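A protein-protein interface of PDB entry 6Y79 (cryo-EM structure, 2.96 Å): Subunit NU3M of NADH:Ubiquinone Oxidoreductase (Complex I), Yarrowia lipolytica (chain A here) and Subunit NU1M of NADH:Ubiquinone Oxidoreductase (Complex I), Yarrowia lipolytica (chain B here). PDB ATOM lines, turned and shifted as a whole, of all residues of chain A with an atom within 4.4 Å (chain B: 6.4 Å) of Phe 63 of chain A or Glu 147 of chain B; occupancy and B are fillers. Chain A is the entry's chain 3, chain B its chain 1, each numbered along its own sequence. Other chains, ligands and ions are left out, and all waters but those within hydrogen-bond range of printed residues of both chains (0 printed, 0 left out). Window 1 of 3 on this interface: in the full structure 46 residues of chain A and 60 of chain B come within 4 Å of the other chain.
The backbone NH (N) of Glu 147 of chain B is in hydrogen-bond range of the side-chain carboxylate (OE1) of Glu 196 of chain B.
The side-chain hydroxyl of Ser 145 of chain B lies within hydrogen-bond range of the indole nitrogen of Trp 313 of chain B, 2.7 Å away.
O of Leu 148 of chain B sits at hydrogen-bond distance from OG of Ser 152 of chain B (2.8 Å).
The backbone carbonyl oxygen of Glu 147 of chain B lies within hydrogen-bond range of the side-chain hydroxyl of Thr 151 of chain B (2.7 Å).
NE1 of Trp 313 of chain B touches CG2 of Val 59 of chain A, 3.5 Å away.
Ile 144 of chain B touches Ala 60 of chain A (CD1 to CB, 3.9 Å).
CZ3 of Trp 313 of chain B touches CD1 of Leu 62 of chain A, at 3.6 Å.
Phe 63 of chain A touches Ile 144 of chain B.
Phe 63 of chain A touches Glu 147 of chain B (CZ to OE2, 3.1 Å).
CE1 of Phe 63 of chain A touches CD1 of Leu 148 of chain B, 3.5 Å away.
CH2 of Trp 313 of chain B touches CA of Phe 63 of chain A, at 3.8 Å.
CB of Phe 66 of chain A touches CD1 of Leu 148 of chain B (3.7 Å).
Trp 313 of chain B touches Phe 66 of chain A.
Of the printed residues of chain B, Val 59 of chain A touches Trp 313 (3.5 Å).
Of chain B, only Ile 144, Glu 147, Leu 148 and Trp 313 come within 4 Å of Phe 63 of chain A.
Leu 143 of chain B touches none of the printed residues of chain A.
Of the printed residues of chain A, Ile 144 of chain B touches Ala 60 (3.9 Å) and Phe 63 (3.1 Å).
Printed residues of chain A within 4 Å of Glu 147 of chain B: Phe 63 (3.1 Å).
Printed residues of chain A within 4 Å of Leu 148 of chain B: Phe 63 and Phe 66.
Printed residues of chain A within 4 Å of Trp 313 of chain B: Val 59, Leu 62, Phe 63 and Phe 66.
The nearest residue of chain B that does not touch Phe 63 of chain A is Ser 145 of chain B (4.4 Å).
The nearest printed residue of chain A that does not touch Glu 147 of chain B is Asp 67 of chain A (4.8 Å).
Among the printed residues, no Asp or Glu carboxylate lies within 4 Å of a Lys or Arg side-chain nitrogen of the other chain.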
ATOM      1  N   VAL A  59       1.037  17.699  -8.748  1.00  0.00           N
ATOM      2  CA  VAL A  59       1.761  18.037  -7.516  1.00  0.00           C
ATOM      3  C   VAL A  59       1.151  17.320  -6.312  1.00  0.00           C
ATOM      4  O   VAL A  59       1.867  16.714  -5.509  1.00  0.00           O
ATOM      5  CB  VAL A  59       1.847  19.568  -7.312  1.00  0.00           C
ATOM      6  CG1 VAL A  59       0.504  20.255  -7.307  1.00  0.00           C
ATOM      7  CG2 VAL A  59       2.572  19.907  -6.026  1.00  0.00           C
ATOM      8  N   ALA A  60      -0.171  17.232  -6.259  1.00  0.00           N
ATOM      9  CA  ALA A  60      -0.812  16.545  -5.152  1.00  0.00           C
ATOM     10  C   ALA A  60      -0.924  15.045  -5.349  1.00  0.00           C
ATOM     11  O   ALA A  60      -1.073  14.326  -4.356  1.00  0.00           O
ATOM     12  CB  ALA A  60      -2.205  17.108  -4.904  1.00  0.00           C
ATOM     13  N   ILE A  61      -0.876  14.534  -6.582  1.00  0.00           N
ATOM     14  CA  ILE A  61      -0.817  13.081  -6.700  1.00  0.00           C
ATOM     15  C   ILE A  61       0.578  12.579  -6.353  1.00  0.00           C
ATOM     16  O   ILE A  61       0.730  11.687  -5.514  1.00  0.00           O
ATOM     17  CB  ILE A  61      -1.271  12.597  -8.086  1.00  0.00           C
ATOM     18  CG1 ILE A  61      -2.753  12.877  -8.295  1.00  0.00           C
ATOM     19  CG2 ILE A  61      -1.130  11.119  -8.156  1.00  0.00           C
ATOM     20  CD1 ILE A  61      -3.244  12.555  -9.687  1.00  0.00           C
ATOM     21  N   LEU A  62       1.628  13.164  -6.944  1.00  0.00           N
ATOM     22  CA  LEU A  62       2.968  12.701  -6.599  1.00  0.00           C
ATOM     23  C   LEU A  62       3.422  13.196  -5.237  1.00  0.00           C
ATOM     24  O   LEU A  62       4.523  12.841  -4.824  1.00  0.00           O
ATOM     25  CB  LEU A  62       4.034  13.090  -7.643  1.00  0.00           C
ATOM     26  CG  LEU A  62       4.530  14.495  -8.020  1.00  0.00           C
ATOM     27  CD1 LEU A  62       5.539  15.132  -7.071  1.00  0.00           C
ATOM     28  CD2 LEU A  62       5.167  14.414  -9.387  1.00  0.00           C
ATOM     29  N   PHE A  63       2.647  14.048  -4.562  1.00  0.00           N
ATOM     30  CA  PHE A  63       2.987  14.430  -3.198  1.00  0.00           C
ATOM     31  C   PHE A  63       3.000  13.235  -2.263  1.00  0.00           C
ATOM     32  O   PHE A  63       3.902  13.097  -1.431  1.00  0.00           O
ATOM     33  CB  PHE A  63       1.994  15.461  -2.677  1.00  0.00           C
ATOM     34  CG  PHE A  63       2.168  15.749  -1.231  1.00  0.00           C
ATOM     35  CD1 PHE A  63       3.292  16.414  -0.808  1.00  0.00           C
ATOM     36  CD2 PHE A  63       1.245  15.320  -0.285  1.00  0.00           C
ATOM     37  CE1 PHE A  63       3.487  16.662   0.512  1.00  0.00           C
ATOM     38  CE2 PHE A  63       1.448  15.576   1.051  1.00  0.00           C
ATOM     39  CZ  PHE A  63       2.574  16.248   1.441  1.00  0.00           C
ATOM     40  N   LEU A  64       2.012  12.381  -2.379  1.00  0.00           N
ATOM     41  CA  LEU A  64       1.762  11.273  -1.467  1.00  0.00           C
ATOM     42  C   LEU A  64       2.852  10.189  -1.435  1.00  0.00           C
ATOM     43  O   LEU A  64       3.139   9.696  -0.338  1.00  0.00           O
ATOM     44  CB  LEU A  64       0.383  10.691  -1.798  1.00  0.00           C
ATOM     45  CG  LEU A  64      -0.338   9.779  -0.822  1.00  0.00           C
ATOM     46  CD1 LEU A  64      -1.823  10.008  -0.914  1.00  0.00           C
ATOM     47  CD2 LEU A  64      -0.036   8.380  -1.200  1.00  0.00           C
ATOM     48  N   PRO A  65       3.473   9.753  -2.550  1.00  0.00           N
ATOM     49  CA  PRO A  65       4.579   8.792  -2.406  1.00  0.00           C
ATOM     50  C   PRO A  65       5.823   9.347  -1.740  1.00  0.00           C
ATOM     51  O   PRO A  65       6.610   8.557  -1.213  1.00  0.00           O
ATOM     52  CB  PRO A  65       4.872   8.382  -3.851  1.00  0.00           C
ATOM     53  CG  PRO A  65       3.606   8.536  -4.511  1.00  0.00           C
ATOM     54  CD  PRO A  65       3.071   9.799  -3.971  1.00  0.00           C
ATOM     55  N   PHE A  66       6.045  10.661  -1.750  1.00  0.00           N
ATOM     56  CA  PHE A  66       7.167  11.196  -0.988  1.00  0.00           C
ATOM     57  C   PHE A  66       6.814  11.293   0.489  1.00  0.00           C
ATOM     58  O   PHE A  66       7.655  11.018   1.350  1.00  0.00           O
ATOM     59  CB  PHE A  66       7.587  12.558  -1.532  1.00  0.00           C
ATOM     60  CG  PHE A  66       8.215  12.512  -2.896  1.00  0.00           C
ATOM     61  CD1 PHE A  66       9.545  12.167  -3.064  1.00  0.00           C
ATOM     62  CD2 PHE A  66       7.481  12.846  -4.010  1.00  0.00           C
ATOM     63  CE1 PHE A  66      10.112  12.143  -4.333  1.00  0.00           C
ATOM     64  CE2 PHE A  66       8.039  12.823  -5.276  1.00  0.00           C
ATOM     65  CZ  PHE A  66       9.351  12.472  -5.436  1.00  0.00           C
ATOM     66  N   ASP A  67       5.565  11.651   0.786  1.00  0.00           N
ATOM     67  CA  ASP A  67       5.069  11.693   2.159  1.00  0.00           C
ATOM     68  C   ASP A  67       5.098  10.317   2.813  1.00  0.00           C
ATOM     69  O   ASP A  67       5.397  10.198   4.006  1.00  0.00           O
ATOM     70  CB  ASP A  67       3.647  12.249   2.161  1.00  0.00           C
ATOM     71  CG  ASP A  67       3.127  12.545   3.546  1.00  0.00           C
ATOM     72  OD1 ASP A  67       3.924  12.616   4.500  1.00  0.00           O
ATOM     73  OD2 ASP A  67       1.899  12.704   3.683  1.00  0.00           O
ATOM     74  N   LEU B 110       3.306  17.011  14.630  1.00  0.00           N
ATOM     75  CA  LEU B 110       3.368  16.730  13.209  1.00  0.00           C
ATOM     76  C   LEU B 110       2.038  16.246  12.650  1.00  0.00           C
ATOM     77  O   LEU B 110       1.751  16.468  11.471  1.00  0.00           O
ATOM     78  CB  LEU B 110       4.449  15.678  12.988  1.00  0.00           C
ATOM     79  CG  LEU B 110       5.035  15.377  11.632  1.00  0.00           C
ATOM     80  CD1 LEU B 110       5.286  16.671  10.910  1.00  0.00           C
ATOM     81  CD2 LEU B 110       6.323  14.631  11.895  1.00  0.00           C
ATOM     82  N   GLY B 113      -0.312  19.555  12.616  1.00  0.00           N
ATOM     83  CA  GLY B 113       0.074  20.428  11.520  1.00  0.00           C
ATOM     84  C   GLY B 113      -0.342  19.947  10.146  1.00  0.00           C
ATOM     85  O   GLY B 113      -0.349  20.745   9.205  1.00  0.00           O
ATOM     86  N   SER B 114      -0.674  18.668  10.005  1.00  0.00           N
ATOM     87  CA  SER B 114      -1.245  18.176   8.763  1.00  0.00           C
ATOM     88  C   SER B 114      -2.759  18.309   8.733  1.00  0.00           C
ATOM     89  O   SER B 114      -3.353  18.224   7.655  1.00  0.00           O
ATOM     90  CB  SER B 114      -0.858  16.717   8.554  1.00  0.00           C
ATOM     91  OG  SER B 114      -1.528  15.895   9.492  1.00  0.00           O
ATOM     92  N   VAL B 117      -4.534  21.798   6.809  1.00  0.00           N
ATOM     93  CA  VAL B 117      -4.718  22.064   5.389  1.00  0.00           C
ATOM     94  C   VAL B 117      -6.193  22.167   5.017  1.00  0.00           C
ATOM     95  O   VAL B 117      -6.532  22.931   4.097  1.00  0.00           O
ATOM     96  CB  VAL B 117      -3.999  20.988   4.554  1.00  0.00           C
ATOM     97  CG1 VAL B 117      -2.513  20.999   4.855  1.00  0.00           C
ATOM     98  CG2 VAL B 117      -4.541  19.615   4.850  1.00  0.00           C
ATOM     99  N   GLN B 142       0.363  24.429  -2.477  1.00  0.00           N
ATOM    100  CA  GLN B 142       1.521  25.016  -1.804  1.00  0.00           C
ATOM    101  C   GLN B 142       1.635  24.545  -0.355  1.00  0.00           C
ATOM    102  O   GLN B 142       2.733  24.219   0.121  1.00  0.00           O
ATOM    103  CB  GLN B 142       1.421  26.536  -1.860  1.00  0.00           C
ATOM    104  CG  GLN B 142       2.221  27.239  -0.791  1.00  0.00           C
ATOM    105  CD  GLN B 142       1.862  28.684  -0.638  1.00  0.00           C
ATOM    106  OE1 GLN B 142       0.872  29.153  -1.186  1.00  0.00           O
ATOM    107  NE2 GLN B 142       2.676  29.408   0.104  1.00  0.00           N
ATOM    108  N   LEU B 143       0.495  24.463   0.336  1.00  0.00           N
ATOM    109  CA  LEU B 143       0.449  24.080   1.746  1.00  0.00           C
ATOM    110  C   LEU B 143       1.025  22.685   1.978  1.00  0.00           C
ATOM    111  O   LEU B 143       1.916  22.495   2.825  1.00  0.00           O
ATOM    112  CB  LEU B 143      -1.004  24.152   2.204  1.00  0.00           C
ATOM    113  CG  LEU B 143      -1.432  24.332   3.648  1.00  0.00           C
ATOM    114  CD1 LEU B 143      -0.554  25.328   4.297  1.00  0.00           C
ATOM    115  CD2 LEU B 143      -2.863  24.826   3.667  1.00  0.00           C
ATOM    116  N   ILE B 144       0.570  21.706   1.190  1.00  0.00           N
ATOM    117  CA  ILE B 144       1.072  20.344   1.344  1.00  0.00           C
ATOM    118  C   ILE B 144       2.519  20.245   0.868  1.00  0.00           C
ATOM    119  O   ILE B 144       3.346  19.572   1.508  1.00  0.00           O
ATOM    120  CB  ILE B 144       0.145  19.326   0.647  1.00  0.00           C
ATOM    121  CG1 ILE B 144       0.058  19.535  -0.866  1.00  0.00           C
ATOM    122  CG2 ILE B 144      -1.238  19.377   1.249  1.00  0.00           C
ATOM    123  CD1 ILE B 144      -0.685  18.465  -1.588  1.00  0.00           C
ATOM    124  N   SER B 145       2.866  20.986  -0.199  1.00  0.00           N
ATOM    125  CA  SER B 145       4.200  20.924  -0.775  1.00  0.00           C
ATOM    126  C   SER B 145       5.260  21.401   0.199  1.00  0.00           C
ATOM    127  O   SER B 145       6.369  20.866   0.213  1.00  0.00           O
ATOM    128  CB  SER B 145       4.230  21.755  -2.055  1.00  0.00           C
ATOM    129  OG  SER B 145       5.512  21.762  -2.645  1.00  0.00           O
ATOM    130  N   TYR B 146       4.924  22.349   1.064  1.00  0.00           N
ATOM    131  CA  TYR B 146       5.922  22.806   2.019  1.00  0.00           C
ATOM    132  C   TYR B 146       5.830  22.123   3.378  1.00  0.00           C
ATOM    133  O   TYR B 146       6.839  22.082   4.102  1.00  0.00           O
ATOM    134  CB  TYR B 146       5.854  24.325   2.149  1.00  0.00           C
ATOM    135  CG  TYR B 146       6.423  25.002   0.922  1.00  0.00           C
ATOM    136  CD1 TYR B 146       7.779  25.246   0.806  1.00  0.00           C
ATOM    137  CD2 TYR B 146       5.603  25.373  -0.128  1.00  0.00           C
ATOM    138  CE1 TYR B 146       8.289  25.851  -0.310  1.00  0.00           C
ATOM    139  CE2 TYR B 146       6.103  25.969  -1.244  1.00  0.00           C
ATOM    140  CZ  TYR B 146       7.444  26.210  -1.329  1.00  0.00           C
ATOM    141  OH  TYR B 146       7.949  26.806  -2.451  1.00  0.00           O
ATOM    142  N   GLU B 147       4.693  21.511   3.731  1.00  0.00           N
ATOM    143  CA  GLU B 147       4.736  20.696   4.945  1.00  0.00           C
ATOM    144  C   GLU B 147       5.484  19.385   4.723  1.00  0.00           C
ATOM    145  O   GLU B 147       5.898  18.747   5.702  1.00  0.00           O
ATOM    146  CB  GLU B 147       3.339  20.436   5.509  1.00  0.00           C
ATOM    147  CG  GLU B 147       2.390  19.663   4.656  1.00  0.00           C
ATOM    148  CD  GLU B 147       2.399  18.189   4.946  1.00  0.00           C
ATOM    149  OE1 GLU B 147       3.036  17.775   5.931  1.00  0.00           O
ATOM    150  OE2 GLU B 147       1.749  17.442   4.198  1.00  0.00           O
ATOM    151  N   LEU B 148       5.688  18.983   3.460  1.00  0.00           N
ATOM    152  CA  LEU B 148       6.640  17.909   3.158  1.00  0.00           C
ATOM    153  C   LEU B 148       8.030  18.204   3.720  1.00  0.00           C
ATOM    154  O   LEU B 148       8.584  17.414   4.496  1.00  0.00           O
ATOM    155  CB  LEU B 148       6.730  17.672   1.644  1.00  0.00           C
ATOM    156  CG  LEU B 148       7.476  16.421   1.128  1.00  0.00           C
ATOM    157  CD1 LEU B 148       6.842  15.881  -0.111  1.00  0.00           C
ATOM    158  CD2 LEU B 148       8.938  16.667   0.811  1.00  0.00           C
ATOM    159  N   ILE B 149       8.619  19.336   3.330  1.00  0.00           N
ATOM    160  CA  ILE B 149       9.978  19.626   3.768  1.00  0.00           C
ATOM    161  C   ILE B 149      10.023  20.037   5.230  1.00  0.00           C
ATOM    162  O   ILE B 149      11.065  19.872   5.879  1.00  0.00           O
ATOM    163  CB  ILE B 149      10.637  20.683   2.861  1.00  0.00           C
ATOM    164  CG1 ILE B 149       9.926  22.015   2.970  1.00  0.00           C
ATOM    165  CG2 ILE B 149      10.627  20.227   1.413  1.00  0.00           C
ATOM    166  CD1 ILE B 149      10.526  23.061   2.110  1.00  0.00           C
ATOM    167  N   LEU B 150       8.898  20.502   5.780  1.00  0.00           N
ATOM    168  CA  LEU B 150       8.777  20.685   7.226  1.00  0.00           C
ATOM    169  C   LEU B 150       8.976  19.370   7.981  1.00  0.00           C
ATOM    170  O   LEU B 150       9.826  19.268   8.885  1.00  0.00           O
ATOM    171  CB  LEU B 150       7.400  21.276   7.520  1.00  0.00           C
ATOM    172  CG  LEU B 150       6.990  21.803   8.883  1.00  0.00           C
ATOM    173  CD1 LEU B 150       7.595  23.165   9.082  1.00  0.00           C
ATOM    174  CD2 LEU B 150       5.476  21.872   8.949  1.00  0.00           C
ATOM    175  N   THR B 151       8.190  18.348   7.608  1.00  0.00           N
ATOM    176  CA  THR B 151       8.307  17.007   8.185  1.00  0.00           C
ATOM    177  C   THR B 151       9.700  16.420   7.985  1.00  0.00           C
ATOM    178  O   THR B 151      10.238  15.744   8.879  1.00  0.00           O
ATOM    179  CB  THR B 151       7.253  16.102   7.549  1.00  0.00           C
ATOM    180  OG1 THR B 151       5.986  16.768   7.568  1.00  0.00           O
ATOM    181  CG2 THR B 151       7.126  14.804   8.294  1.00  0.00           C
ATOM    182  N   SER B 152      10.305  16.703   6.827  1.00  0.00           N
ATOM    183  CA  SER B 152      11.653  16.230   6.539  1.00  0.00           C
ATOM    184  C   SER B 152      12.672  16.804   7.515  1.00  0.00           C
ATOM    185  O   SER B 152      13.519  16.066   8.028  1.00  0.00           O
ATOM    186  CB  SER B 152      12.026  16.608   5.118  1.00  0.00           C
ATOM    187  OG  SER B 152      11.089  16.100   4.178  1.00  0.00           O
ATOM    188  N   ALA B 192      10.582  27.353   4.965  1.00  0.00           N
ATOM    189  CA  ALA B 192       9.453  26.425   4.949  1.00  0.00           C
ATOM    190  C   ALA B 192       8.381  26.823   5.952  1.00  0.00           C
ATOM    191  O   ALA B 192       7.189  26.616   5.700  1.00  0.00           O
ATOM    192  CB  ALA B 192       9.933  25.009   5.234  1.00  0.00           C
ATOM    193  N   GLU B 196       4.517  27.698   5.110  1.00  0.00           N
ATOM    194  CA  GLU B 196       3.464  26.858   5.671  1.00  0.00           C
ATOM    195  C   GLU B 196       2.301  27.674   6.232  1.00  0.00           C
ATOM    196  O   GLU B 196       1.174  27.177   6.311  1.00  0.00           O
ATOM    197  CB  GLU B 196       4.081  25.929   6.723  1.00  0.00           C
ATOM    198  CG  GLU B 196       3.161  24.909   7.401  1.00  0.00           C
ATOM    199  CD  GLU B 196       2.533  23.905   6.448  1.00  0.00           C
ATOM    200  OE1 GLU B 196       3.070  23.679   5.346  1.00  0.00           O
ATOM    201  OE2 GLU B 196       1.493  23.325   6.819  1.00  0.00           O
ATOM    202  N   TRP B 313       9.991  21.743  -5.190  1.00  0.00           N
ATOM    203  CA  TRP B 313      10.220  20.384  -5.654  1.00  0.00           C
ATOM    204  C   TRP B 313      11.528  20.225  -6.404  1.00  0.00           C
ATOM    205  O   TRP B 313      12.072  19.119  -6.447  1.00  0.00           O
ATOM    206  CB  TRP B 313       9.059  19.943  -6.535  1.00  0.00           C
ATOM    207  CG  TRP B 313       7.811  19.769  -5.773  1.00  0.00           C
ATOM    208  CD1 TRP B 313       6.843  20.694  -5.572  1.00  0.00           C
ATOM    209  CD2 TRP B 313       7.387  18.590  -5.092  1.00  0.00           C
ATOM    210  NE1 TRP B 313       5.838  20.170  -4.809  1.00  0.00           N
ATOM    211  CE2 TRP B 313       6.148  18.874  -4.500  1.00  0.00           C
ATOM    212  CE3 TRP B 313       7.936  17.317  -4.928  1.00  0.00           C
ATOM    213  CZ2 TRP B 313       5.447  17.936  -3.753  1.00  0.00           C
ATOM    214  CZ3 TRP B 313       7.245  16.391  -4.181  1.00  0.00           C
ATOM    215  CH2 TRP B 313       6.010  16.701  -3.606  1.00  0.00           C
